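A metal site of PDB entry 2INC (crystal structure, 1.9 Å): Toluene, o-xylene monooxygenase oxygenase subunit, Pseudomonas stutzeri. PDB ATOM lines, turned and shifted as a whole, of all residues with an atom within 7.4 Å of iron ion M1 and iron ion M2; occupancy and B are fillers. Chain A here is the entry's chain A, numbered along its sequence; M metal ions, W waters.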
ATOM      1  N   ILE A  99      22.314 -20.665  -5.130  1.00  0.00           N
ATOM      2  CA  ILE A  99      23.021 -19.668  -4.306  1.00  0.00           C
ATOM      3  C   ILE A  99      23.297 -20.063  -2.860  1.00  0.00           C
ATOM      4  O   ILE A  99      24.322 -19.665  -2.318  1.00  0.00           O
ATOM      5  CB  ILE A  99      22.217 -18.318  -4.486  1.00  0.00           C
ATOM      6  CG1 ILE A  99      22.746 -17.630  -5.760  1.00  0.00           C
ATOM      7  CG2 ILE A  99      22.215 -17.381  -3.293  1.00  0.00           C
ATOM      8  CD1 ILE A  99      24.163 -18.006  -6.086  1.00  0.00           C
ATOM      9  N   GLU A 102      26.766 -21.652  -2.293  1.00  0.00           N
ATOM     10  CA  GLU A 102      27.787 -20.695  -2.820  1.00  0.00           C
ATOM     11  C   GLU A 102      27.959 -19.435  -1.961  1.00  0.00           C
ATOM     12  O   GLU A 102      29.091 -18.954  -1.810  1.00  0.00           O
ATOM     13  CB  GLU A 102      27.499 -20.330  -4.277  1.00  0.00           C
ATOM     14  CG  GLU A 102      27.520 -21.595  -5.261  1.00  0.00           C
ATOM     15  CD  GLU A 102      28.898 -22.252  -5.416  1.00  0.00           C
ATOM     16  OE1 GLU A 102      29.840 -22.010  -4.615  1.00  0.00           O
ATOM     17  OE2 GLU A 102      29.102 -23.033  -6.372  1.00  0.00           O
ATOM     18  N   GLU A 103      26.865 -18.932  -1.392  1.00  0.00           N
ATOM     19  CA  GLU A 103      26.978 -17.897  -0.269  1.00  0.00           C
ATOM     20  C   GLU A 103      27.879 -18.432   0.826  1.00  0.00           C
ATOM     21  O   GLU A 103      28.862 -17.794   1.225  1.00  0.00           O
ATOM     22  CB  GLU A 103      25.620 -17.574   0.345  1.00  0.00           C
ATOM     23  CG  GLU A 103      24.624 -16.895  -0.621  1.00  0.00           C
ATOM     24  CD  GLU A 103      24.735 -15.376  -0.609  1.00  0.00           C
ATOM     25  OE1 GLU A 103      25.816 -14.793  -0.293  1.00  0.00           O
ATOM     26  OE2 GLU A 103      23.717 -14.740  -0.938  1.00  0.00           O
ATOM     27  N   TYR A 104      27.572 -19.639   1.313  1.00  0.00           N
ATOM     28  CA  TYR A 104      28.406 -20.229   2.357  1.00  0.00           C
ATOM     29  C   TYR A 104      29.870 -20.437   1.940  1.00  0.00           C
ATOM     30  O   TYR A 104      30.812 -20.145   2.733  1.00  0.00           O
ATOM     31  CB  TYR A 104      27.775 -21.537   2.890  1.00  0.00           C
ATOM     32  CG  TYR A 104      28.568 -22.123   4.014  1.00  0.00           C
ATOM     33  CD1 TYR A 104      28.481 -21.593   5.307  1.00  0.00           C
ATOM     34  CD2 TYR A 104      29.365 -23.252   3.799  1.00  0.00           C
ATOM     35  CE1 TYR A 104      29.225 -22.156   6.348  1.00  0.00           C
ATOM     36  CE2 TYR A 104      30.135 -23.822   4.816  1.00  0.00           C
ATOM     37  CZ  TYR A 104      30.051 -23.279   6.091  1.00  0.00           C
ATOM     38  OH  TYR A 104      30.818 -23.829   7.095  1.00  0.00           O
ATOM     39  N   ALA A 106      31.431 -18.590  -0.155  1.00  0.00           N
ATOM     40  CA  ALA A 106      31.973 -17.232  -0.130  1.00  0.00           C
ATOM     41  C   ALA A 106      32.567 -16.887   1.254  1.00  0.00           C
ATOM     42  O   ALA A 106      33.470 -16.035   1.354  1.00  0.00           O
ATOM     43  CB  ALA A 106      30.919 -16.258  -0.544  1.00  0.00           C
ATOM     44  N   GLU A 110      36.172 -15.264   1.655  1.00  0.00           N
ATOM     45  CA  GLU A 110      36.501 -14.113   2.554  1.00  0.00           C
ATOM     46  C   GLU A 110      37.646 -14.528   3.510  1.00  0.00           C
ATOM     47  O   GLU A 110      38.593 -13.760   3.738  1.00  0.00           O
ATOM     48  CB  GLU A 110      35.231 -13.635   3.278  1.00  0.00           C
ATOM     49  CG  GLU A 110      34.185 -12.960   2.319  1.00  0.00           C
ATOM     50  CD  GLU A 110      34.539 -11.486   1.959  1.00  0.00           C
ATOM     51  OE1 GLU A 110      35.471 -10.939   2.602  1.00  0.00           O
ATOM     52  OE2 GLU A 110      33.909 -10.833   1.072  1.00  0.00           O
ATOM     53  N   GLY A 129      33.368  -9.784   6.284  1.00  0.00           N
ATOM     54  CA  GLY A 129      32.810 -10.487   5.086  1.00  0.00           C
ATOM     55  C   GLY A 129      32.568 -11.967   5.328  1.00  0.00           C
ATOM     56  O   GLY A 129      31.542 -12.554   4.905  1.00  0.00           O
ATOM     57  N   ASP A 132      29.460 -12.195   7.281  1.00  0.00           N
ATOM     58  CA  ASP A 132      28.283 -11.894   6.445  1.00  0.00           C
ATOM     59  C   ASP A 132      27.834 -13.064   5.551  1.00  0.00           C
ATOM     60  O   ASP A 132      26.664 -13.388   5.517  1.00  0.00           O
ATOM     61  CB  ASP A 132      28.609 -10.742   5.481  1.00  0.00           C
ATOM     62  CG  ASP A 132      28.716  -9.397   6.178  1.00  0.00           C
ATOM     63  OD1 ASP A 132      28.218  -9.272   7.325  1.00  0.00           O
ATOM     64  OD2 ASP A 132      29.317  -8.478   5.554  1.00  0.00           O
ATOM     65  N   GLU A 133      28.793 -13.693   4.856  1.00  0.00           N
ATOM     66  CA  GLU A 133      28.459 -14.847   4.004  1.00  0.00           C
ATOM     67  C   GLU A 133      28.029 -16.044   4.824  1.00  0.00           C
ATOM     68  O   GLU A 133      27.206 -16.867   4.408  1.00  0.00           O
ATOM     69  CB  GLU A 133      29.652 -15.190   3.119  1.00  0.00           C
ATOM     70  CG  GLU A 133      30.201 -13.987   2.311  1.00  0.00           C
ATOM     71  CD  GLU A 133      29.234 -13.381   1.291  1.00  0.00           C
ATOM     72  OE1 GLU A 133      28.049 -13.678   1.335  1.00  0.00           O
ATOM     73  OE2 GLU A 133      29.658 -12.567   0.424  1.00  0.00           O
ATOM     74  N   ASN A 134      28.573 -16.164   6.023  1.00  0.00           N
ATOM     75  CA  ASN A 134      28.031 -17.146   6.977  1.00  0.00           C
ATOM     76  C   ASN A 134      26.540 -16.914   7.222  1.00  0.00           C
ATOM     77  O   ASN A 134      25.711 -17.838   7.106  1.00  0.00           O
ATOM     78  CB  ASN A 134      28.851 -17.080   8.257  1.00  0.00           C
ATOM     79  CG  ASN A 134      28.359 -18.077   9.305  1.00  0.00           C
ATOM     80  OD1 ASN A 134      27.500 -17.735  10.112  1.00  0.00           O
ATOM     81  ND2 ASN A 134      28.908 -19.299   9.299  1.00  0.00           N
ATOM     82  N   ARG A 135      26.162 -15.657   7.504  1.00  0.00           N
ATOM     83  CA  ARG A 135      24.774 -15.302   7.643  1.00  0.00           C
ATOM     84  C   ARG A 135      23.994 -15.712   6.390  1.00  0.00           C
ATOM     85  O   ARG A 135      22.928 -16.350   6.471  1.00  0.00           O
ATOM     86  CB  ARG A 135      24.594 -13.813   7.821  1.00  0.00           C
ATOM     87  CG  ARG A 135      23.132 -13.375   7.861  1.00  0.00           C
ATOM     88  CD  ARG A 135      22.973 -11.903   8.051  1.00  0.00           C
ATOM     89  NE  ARG A 135      21.559 -11.594   8.347  1.00  0.00           N
ATOM     90  CZ  ARG A 135      20.807 -10.650   7.739  1.00  0.00           C
ATOM     91  NH1 ARG A 135      21.308  -9.815   6.851  1.00  0.00           N
ATOM     92  NH2 ARG A 135      19.552 -10.496   8.109  1.00  0.00           N
ATOM     93  N   HIS A 136      24.489 -15.310   5.230  1.00  0.00           N
ATOM     94  CA  HIS A 136      23.749 -15.500   3.982  1.00  0.00           C
ATOM     95  C   HIS A 136      23.516 -16.954   3.645  1.00  0.00           C
ATOM     96  O   HIS A 136      22.447 -17.295   3.160  1.00  0.00           O
ATOM     97  CB  HIS A 136      24.421 -14.739   2.811  1.00  0.00           C
ATOM     98  CG  HIS A 136      24.543 -13.248   3.052  1.00  0.00           C
ATOM     99  ND1 HIS A 136      25.220 -12.379   2.187  1.00  0.00           N
ATOM    100  CD2 HIS A 136      24.039 -12.467   4.039  1.00  0.00           C
ATOM    101  CE1 HIS A 136      25.168 -11.161   2.683  1.00  0.00           C
ATOM    102  NE2 HIS A 136      24.424 -11.173   3.781  1.00  0.00           N
ATOM    103  N   GLY A 137      24.499 -17.787   3.891  1.00  0.00           N
ATOM    104  CA  GLY A 137      24.377 -19.183   3.591  1.00  0.00           C
ATOM    105  C   GLY A 137      23.366 -19.726   4.569  1.00  0.00           C
ATOM    106  O   GLY A 137      22.485 -20.502   4.184  1.00  0.00           O
ATOM    107  N   GLN A 140      19.582 -18.406   4.002  1.00  0.00           N
ATOM    108  CA  GLN A 140      19.077 -18.903   2.730  1.00  0.00           C
ATOM    109  C   GLN A 140      18.946 -20.422   2.738  1.00  0.00           C
ATOM    110  O   GLN A 140      18.558 -21.033   1.723  1.00  0.00           O
ATOM    111  CB  GLN A 140      19.913 -18.418   1.553  1.00  0.00           C
ATOM    112  CG  GLN A 140      19.548 -16.903   1.430  1.00  0.00           C
ATOM    113  CD  GLN A 140      20.239 -16.173   0.288  1.00  0.00           C
ATOM    114  OE1 GLN A 140      19.594 -15.814  -0.682  1.00  0.00           O
ATOM    115  NE2 GLN A 140      21.532 -15.971   0.410  1.00  0.00           N
ATOM    116  N   LEU A 191      35.848 -11.431  -7.024  1.00  0.00           N
ATOM    117  CA  LEU A 191      34.615 -11.571  -6.232  1.00  0.00           C
ATOM    118  C   LEU A 191      34.011 -10.197  -5.817  1.00  0.00           C
ATOM    119  O   LEU A 191      32.876  -9.843  -6.204  1.00  0.00           O
ATOM    120  CB  LEU A 191      34.882 -12.444  -4.992  1.00  0.00           C
ATOM    121  CG  LEU A 191      33.749 -12.633  -3.981  1.00  0.00           C
ATOM    122  CD1 LEU A 191      32.521 -13.238  -4.681  1.00  0.00           C
ATOM    123  CD2 LEU A 191      34.160 -13.408  -2.699  1.00  0.00           C
ATOM    124  N   THR A 192      34.746  -9.420  -5.019  1.00  0.00           N
ATOM    125  CA  THR A 192      34.068  -8.330  -4.356  1.00  0.00           C
ATOM    126  C   THR A 192      33.817  -7.141  -5.284  1.00  0.00           C
ATOM    127  O   THR A 192      32.756  -6.536  -5.194  1.00  0.00           O
ATOM    128  CB  THR A 192      34.725  -7.896  -3.007  1.00  0.00           C
ATOM    129  OG1 THR A 192      35.951  -7.221  -3.257  1.00  0.00           O
ATOM    130  CG2 THR A 192      35.042  -9.072  -2.101  1.00  0.00           C
ATOM    131  N   PHE A 195      32.042  -9.078  -9.229  1.00  0.00           N
ATOM    132  CA  PHE A 195      30.769  -9.758  -9.059  1.00  0.00           C
ATOM    133  C   PHE A 195      29.846  -9.089  -8.046  1.00  0.00           C
ATOM    134  O   PHE A 195      28.635  -8.951  -8.280  1.00  0.00           O
ATOM    135  CB  PHE A 195      31.010 -11.220  -8.622  1.00  0.00           C
ATOM    136  CG  PHE A 195      29.748 -12.063  -8.527  1.00  0.00           C
ATOM    137  CD1 PHE A 195      28.973 -12.340  -9.658  1.00  0.00           C
ATOM    138  CD2 PHE A 195      29.372 -12.620  -7.325  1.00  0.00           C
ATOM    139  CE1 PHE A 195      27.827 -13.144  -9.582  1.00  0.00           C
ATOM    140  CE2 PHE A 195      28.231 -13.409  -7.244  1.00  0.00           C
ATOM    141  CZ  PHE A 195      27.476 -13.689  -8.364  1.00  0.00           C
ATOM    142  N   GLU A 196      30.346  -8.744  -6.865  1.00  0.00           N
ATOM    143  CA  GLU A 196      29.413  -8.295  -5.815  1.00  0.00           C
ATOM    144  C   GLU A 196      29.058  -6.815  -6.011  1.00  0.00           C
ATOM    145  O   GLU A 196      27.865  -6.416  -6.076  1.00  0.00           O
ATOM    146  CB  GLU A 196      29.989  -8.548  -4.399  1.00  0.00           C
ATOM    147  CG  GLU A 196      30.133 -10.039  -4.005  1.00  0.00           C
ATOM    148  CD  GLU A 196      30.670 -10.231  -2.578  1.00  0.00           C
ATOM    149  OE1 GLU A 196      31.724  -9.653  -2.290  1.00  0.00           O
ATOM    150  OE2 GLU A 196      30.070 -10.959  -1.742  1.00  0.00           O
ATOM    151  N   THR A 200      25.706  -8.183  -8.050  1.00  0.00           N
ATOM    152  CA  THR A 200      24.691  -8.680  -7.105  1.00  0.00           C
ATOM    153  C   THR A 200      24.100  -7.588  -6.206  1.00  0.00           C
ATOM    154  O   THR A 200      22.992  -7.741  -5.694  1.00  0.00           O
ATOM    155  CB  THR A 200      25.208  -9.831  -6.225  1.00  0.00           C
ATOM    156  OG1 THR A 200      26.264  -9.362  -5.420  1.00  0.00           O
ATOM    157  CG2 THR A 200      25.761 -10.921  -7.061  1.00  0.00           C
ATOM    158  N   PHE A 204      20.137  -7.666  -6.246  1.00  0.00           N
ATOM    159  CA  PHE A 204      19.333  -7.991  -5.074  1.00  0.00           C
ATOM    160  C   PHE A 204      18.275  -6.929  -4.755  1.00  0.00           C
ATOM    161  O   PHE A 204      17.216  -7.250  -4.257  1.00  0.00           O
ATOM    162  CB  PHE A 204      20.235  -8.280  -3.859  1.00  0.00           C
ATOM    163  CG  PHE A 204      20.646  -9.725  -3.737  1.00  0.00           C
ATOM    164  CD1 PHE A 204      20.980 -10.487  -4.873  1.00  0.00           C
ATOM    165  CD2 PHE A 204      20.729 -10.336  -2.470  1.00  0.00           C
ATOM    166  CE1 PHE A 204      21.350 -11.865  -4.752  1.00  0.00           C
ATOM    167  CE2 PHE A 204      21.115 -11.698  -2.353  1.00  0.00           C
ATOM    168  CZ  PHE A 204      21.436 -12.463  -3.504  1.00  0.00           C
ATOM    169  N   ILE A 226      19.684  -9.068   3.200  1.00  0.00           N
ATOM    170  CA  ILE A 226      20.960  -9.604   2.772  1.00  0.00           C
ATOM    171  C   ILE A 226      21.627  -8.541   2.004  1.00  0.00           C
ATOM    172  O   ILE A 226      22.809  -8.367   2.110  1.00  0.00           O
ATOM    173  CB  ILE A 226      20.754 -10.765   1.704  1.00  0.00           C
ATOM    174  CG1 ILE A 226      20.275 -12.048   2.338  1.00  0.00           C
ATOM    175  CG2 ILE A 226      22.019 -10.989   0.868  1.00  0.00           C
ATOM    176  CD1 ILE A 226      20.282 -11.998   3.814  1.00  0.00           C
ATOM    177  N   ASP A 229      23.894  -5.954   3.613  1.00  0.00           N
ATOM    178  CA  ASP A 229      25.211  -6.416   4.099  1.00  0.00           C
ATOM    179  C   ASP A 229      26.278  -6.296   3.037  1.00  0.00           C
ATOM    180  O   ASP A 229      27.437  -6.338   3.372  1.00  0.00           O
ATOM    181  CB  ASP A 229      25.178  -7.897   4.491  1.00  0.00           C
ATOM    182  CG  ASP A 229      24.308  -8.185   5.676  1.00  0.00           C
ATOM    183  OD1 ASP A 229      24.118  -7.338   6.565  1.00  0.00           O
ATOM    184  OD2 ASP A 229      23.799  -9.324   5.744  1.00  0.00           O
ATOM    185  N   GLU A 230      25.882  -6.261   1.757  1.00  0.00           N
ATOM    186  CA  GLU A 230      26.774  -6.428   0.638  1.00  0.00           C
ATOM    187  C   GLU A 230      27.893  -5.426   0.578  1.00  0.00           C
ATOM    188  O   GLU A 230      29.059  -5.819   0.501  1.00  0.00           O
ATOM    189  CB  GLU A 230      26.012  -6.474  -0.714  1.00  0.00           C
ATOM    190  CG  GLU A 230      26.834  -7.154  -1.824  1.00  0.00           C
ATOM    191  CD  GLU A 230      26.905  -8.667  -1.591  1.00  0.00           C
ATOM    192  OE1 GLU A 230      25.850  -9.272  -1.238  1.00  0.00           O
ATOM    193  OE2 GLU A 230      28.003  -9.252  -1.734  1.00  0.00           O
ATOM    194  N   SER A 231      27.575  -4.132   0.645  1.00  0.00           N
ATOM    195  CA  SER A 231      28.633  -3.149   0.439  1.00  0.00           C
ATOM    196  C   SER A 231      29.753  -3.213   1.518  1.00  0.00           C
ATOM    197  O   SER A 231      30.907  -2.933   1.244  1.00  0.00           O
ATOM    198  CB  SER A 231      28.053  -1.756   0.332  1.00  0.00           C
ATOM    199  OG  SER A 231      27.617  -1.376   1.621  1.00  0.00           O
ATOM    200  N   HIS A 233      31.361  -5.583   2.506  1.00  0.00           N
ATOM    201  CA  HIS A 233      32.463  -6.457   2.083  1.00  0.00           C
ATOM    202  C   HIS A 233      32.758  -6.340   0.611  1.00  0.00           C
ATOM    203  O   HIS A 233      33.834  -6.630   0.213  1.00  0.00           O
ATOM    204  CB  HIS A 233      32.284  -7.912   2.537  1.00  0.00           C
ATOM    205  CG  HIS A 233      31.077  -8.595   1.970  1.00  0.00           C
ATOM    206  ND1 HIS A 233      29.902  -8.746   2.668  1.00  0.00           N
ATOM    207  CD2 HIS A 233      30.860  -9.165   0.747  1.00  0.00           C
ATOM    208  CE1 HIS A 233      29.020  -9.384   1.913  1.00  0.00           C
ATOM    209  NE2 HIS A 233      29.587  -9.654   0.744  1.00  0.00           N
ATOM    210  N   ALA A 234      31.794  -5.878  -0.191  1.00  0.00           N
ATOM    211  CA  ALA A 234      31.975  -5.748  -1.629  1.00  0.00           C
ATOM    212  C   ALA A 234      32.954  -4.645  -1.908  1.00  0.00           C
ATOM    213  O   ALA A 234      33.610  -4.649  -2.935  1.00  0.00           O
ATOM    214  CB  ALA A 234      30.657  -5.443  -2.264  1.00  0.00           C
HETATM  215 FE    FE M   1      26.334 -12.858   0.296  1.00  0.00          FE
HETATM  216 FE    FE M   2      28.668 -11.038  -0.624  1.00  0.00          FE
HETATM  217  O   HOH W   1      27.696 -12.841  -1.684  1.00  0.00           O
HETATM  218  O   HOH W   2      24.584 -12.205  -0.968  1.00  0.00           O
HETATM  219  O   HOH W   3      27.003 -10.870   0.126  1.00  0.00           O
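Water W2 lies within hydrogen-bond range of the side-chain carboxylate (OE2) of Glu 103 (2.7 Å) and the side-chain carboxylate (OE1) of Glu 230 (3.2 Å).
OE2 of Glu 196 is bound to iron ion M2 (1.8 Å).
Water W3 binds iron ion M2 (1.8 Å).
OE2 of Glu 133 binds iron ion M2, 2.1 Å away.
Iron ion M2 is bound by a ring nitrogen (NE2) of His 233, at 2.2 Å.
OE2 of Glu 230 is bound to iron ion M2, at 2.2 Å.
Water W1 binds iron ion M2, 2.3 Å away.
Four residues have an atom within 4 Å of iron ion M2: Glu 133, Glu 196, Glu 230 and His 233.
The nearest printed residue that does not touch iron ion M1 is His 233 (4.6 Å).
Iron ion M1 is bound by OE1 of Glu 103 (2.1 Å), water W3 (2.1 Å), OE1 of Glu 133 (2.2 Å), ND1 of His 136 (2.2 Å), water W2 (2.3 Å) and water W1 (2.4 Å).
ND1 of His 233 sits at hydrogen-bond distance from OD2 of Asp 132 (3.0 Å).
The backbone carbonyl oxygen (O) of Leu 191 sits at hydrogen-bond distance from the backbone NH (N) of Glu 196.
NE2 of Gln 140 is in hydrogen-bond range of O of His 136, 3.2 Å away.
A ring nitrogen (NE2) of His 136 is in hydrogen-bond range of the side-chain carboxylate (OD2) of Asp 229, at 2.8 Å.
The side-chain hydroxyl of Thr 200 lies close to the backbone carbonyl oxygen of Glu 196 (3.4 Å).
The side-chain carboxylate (OE2) of Glu 103 is in hydrogen-bond range of the side-chain amide nitrogen (NE2) of Gln 140 (2.8 Å).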
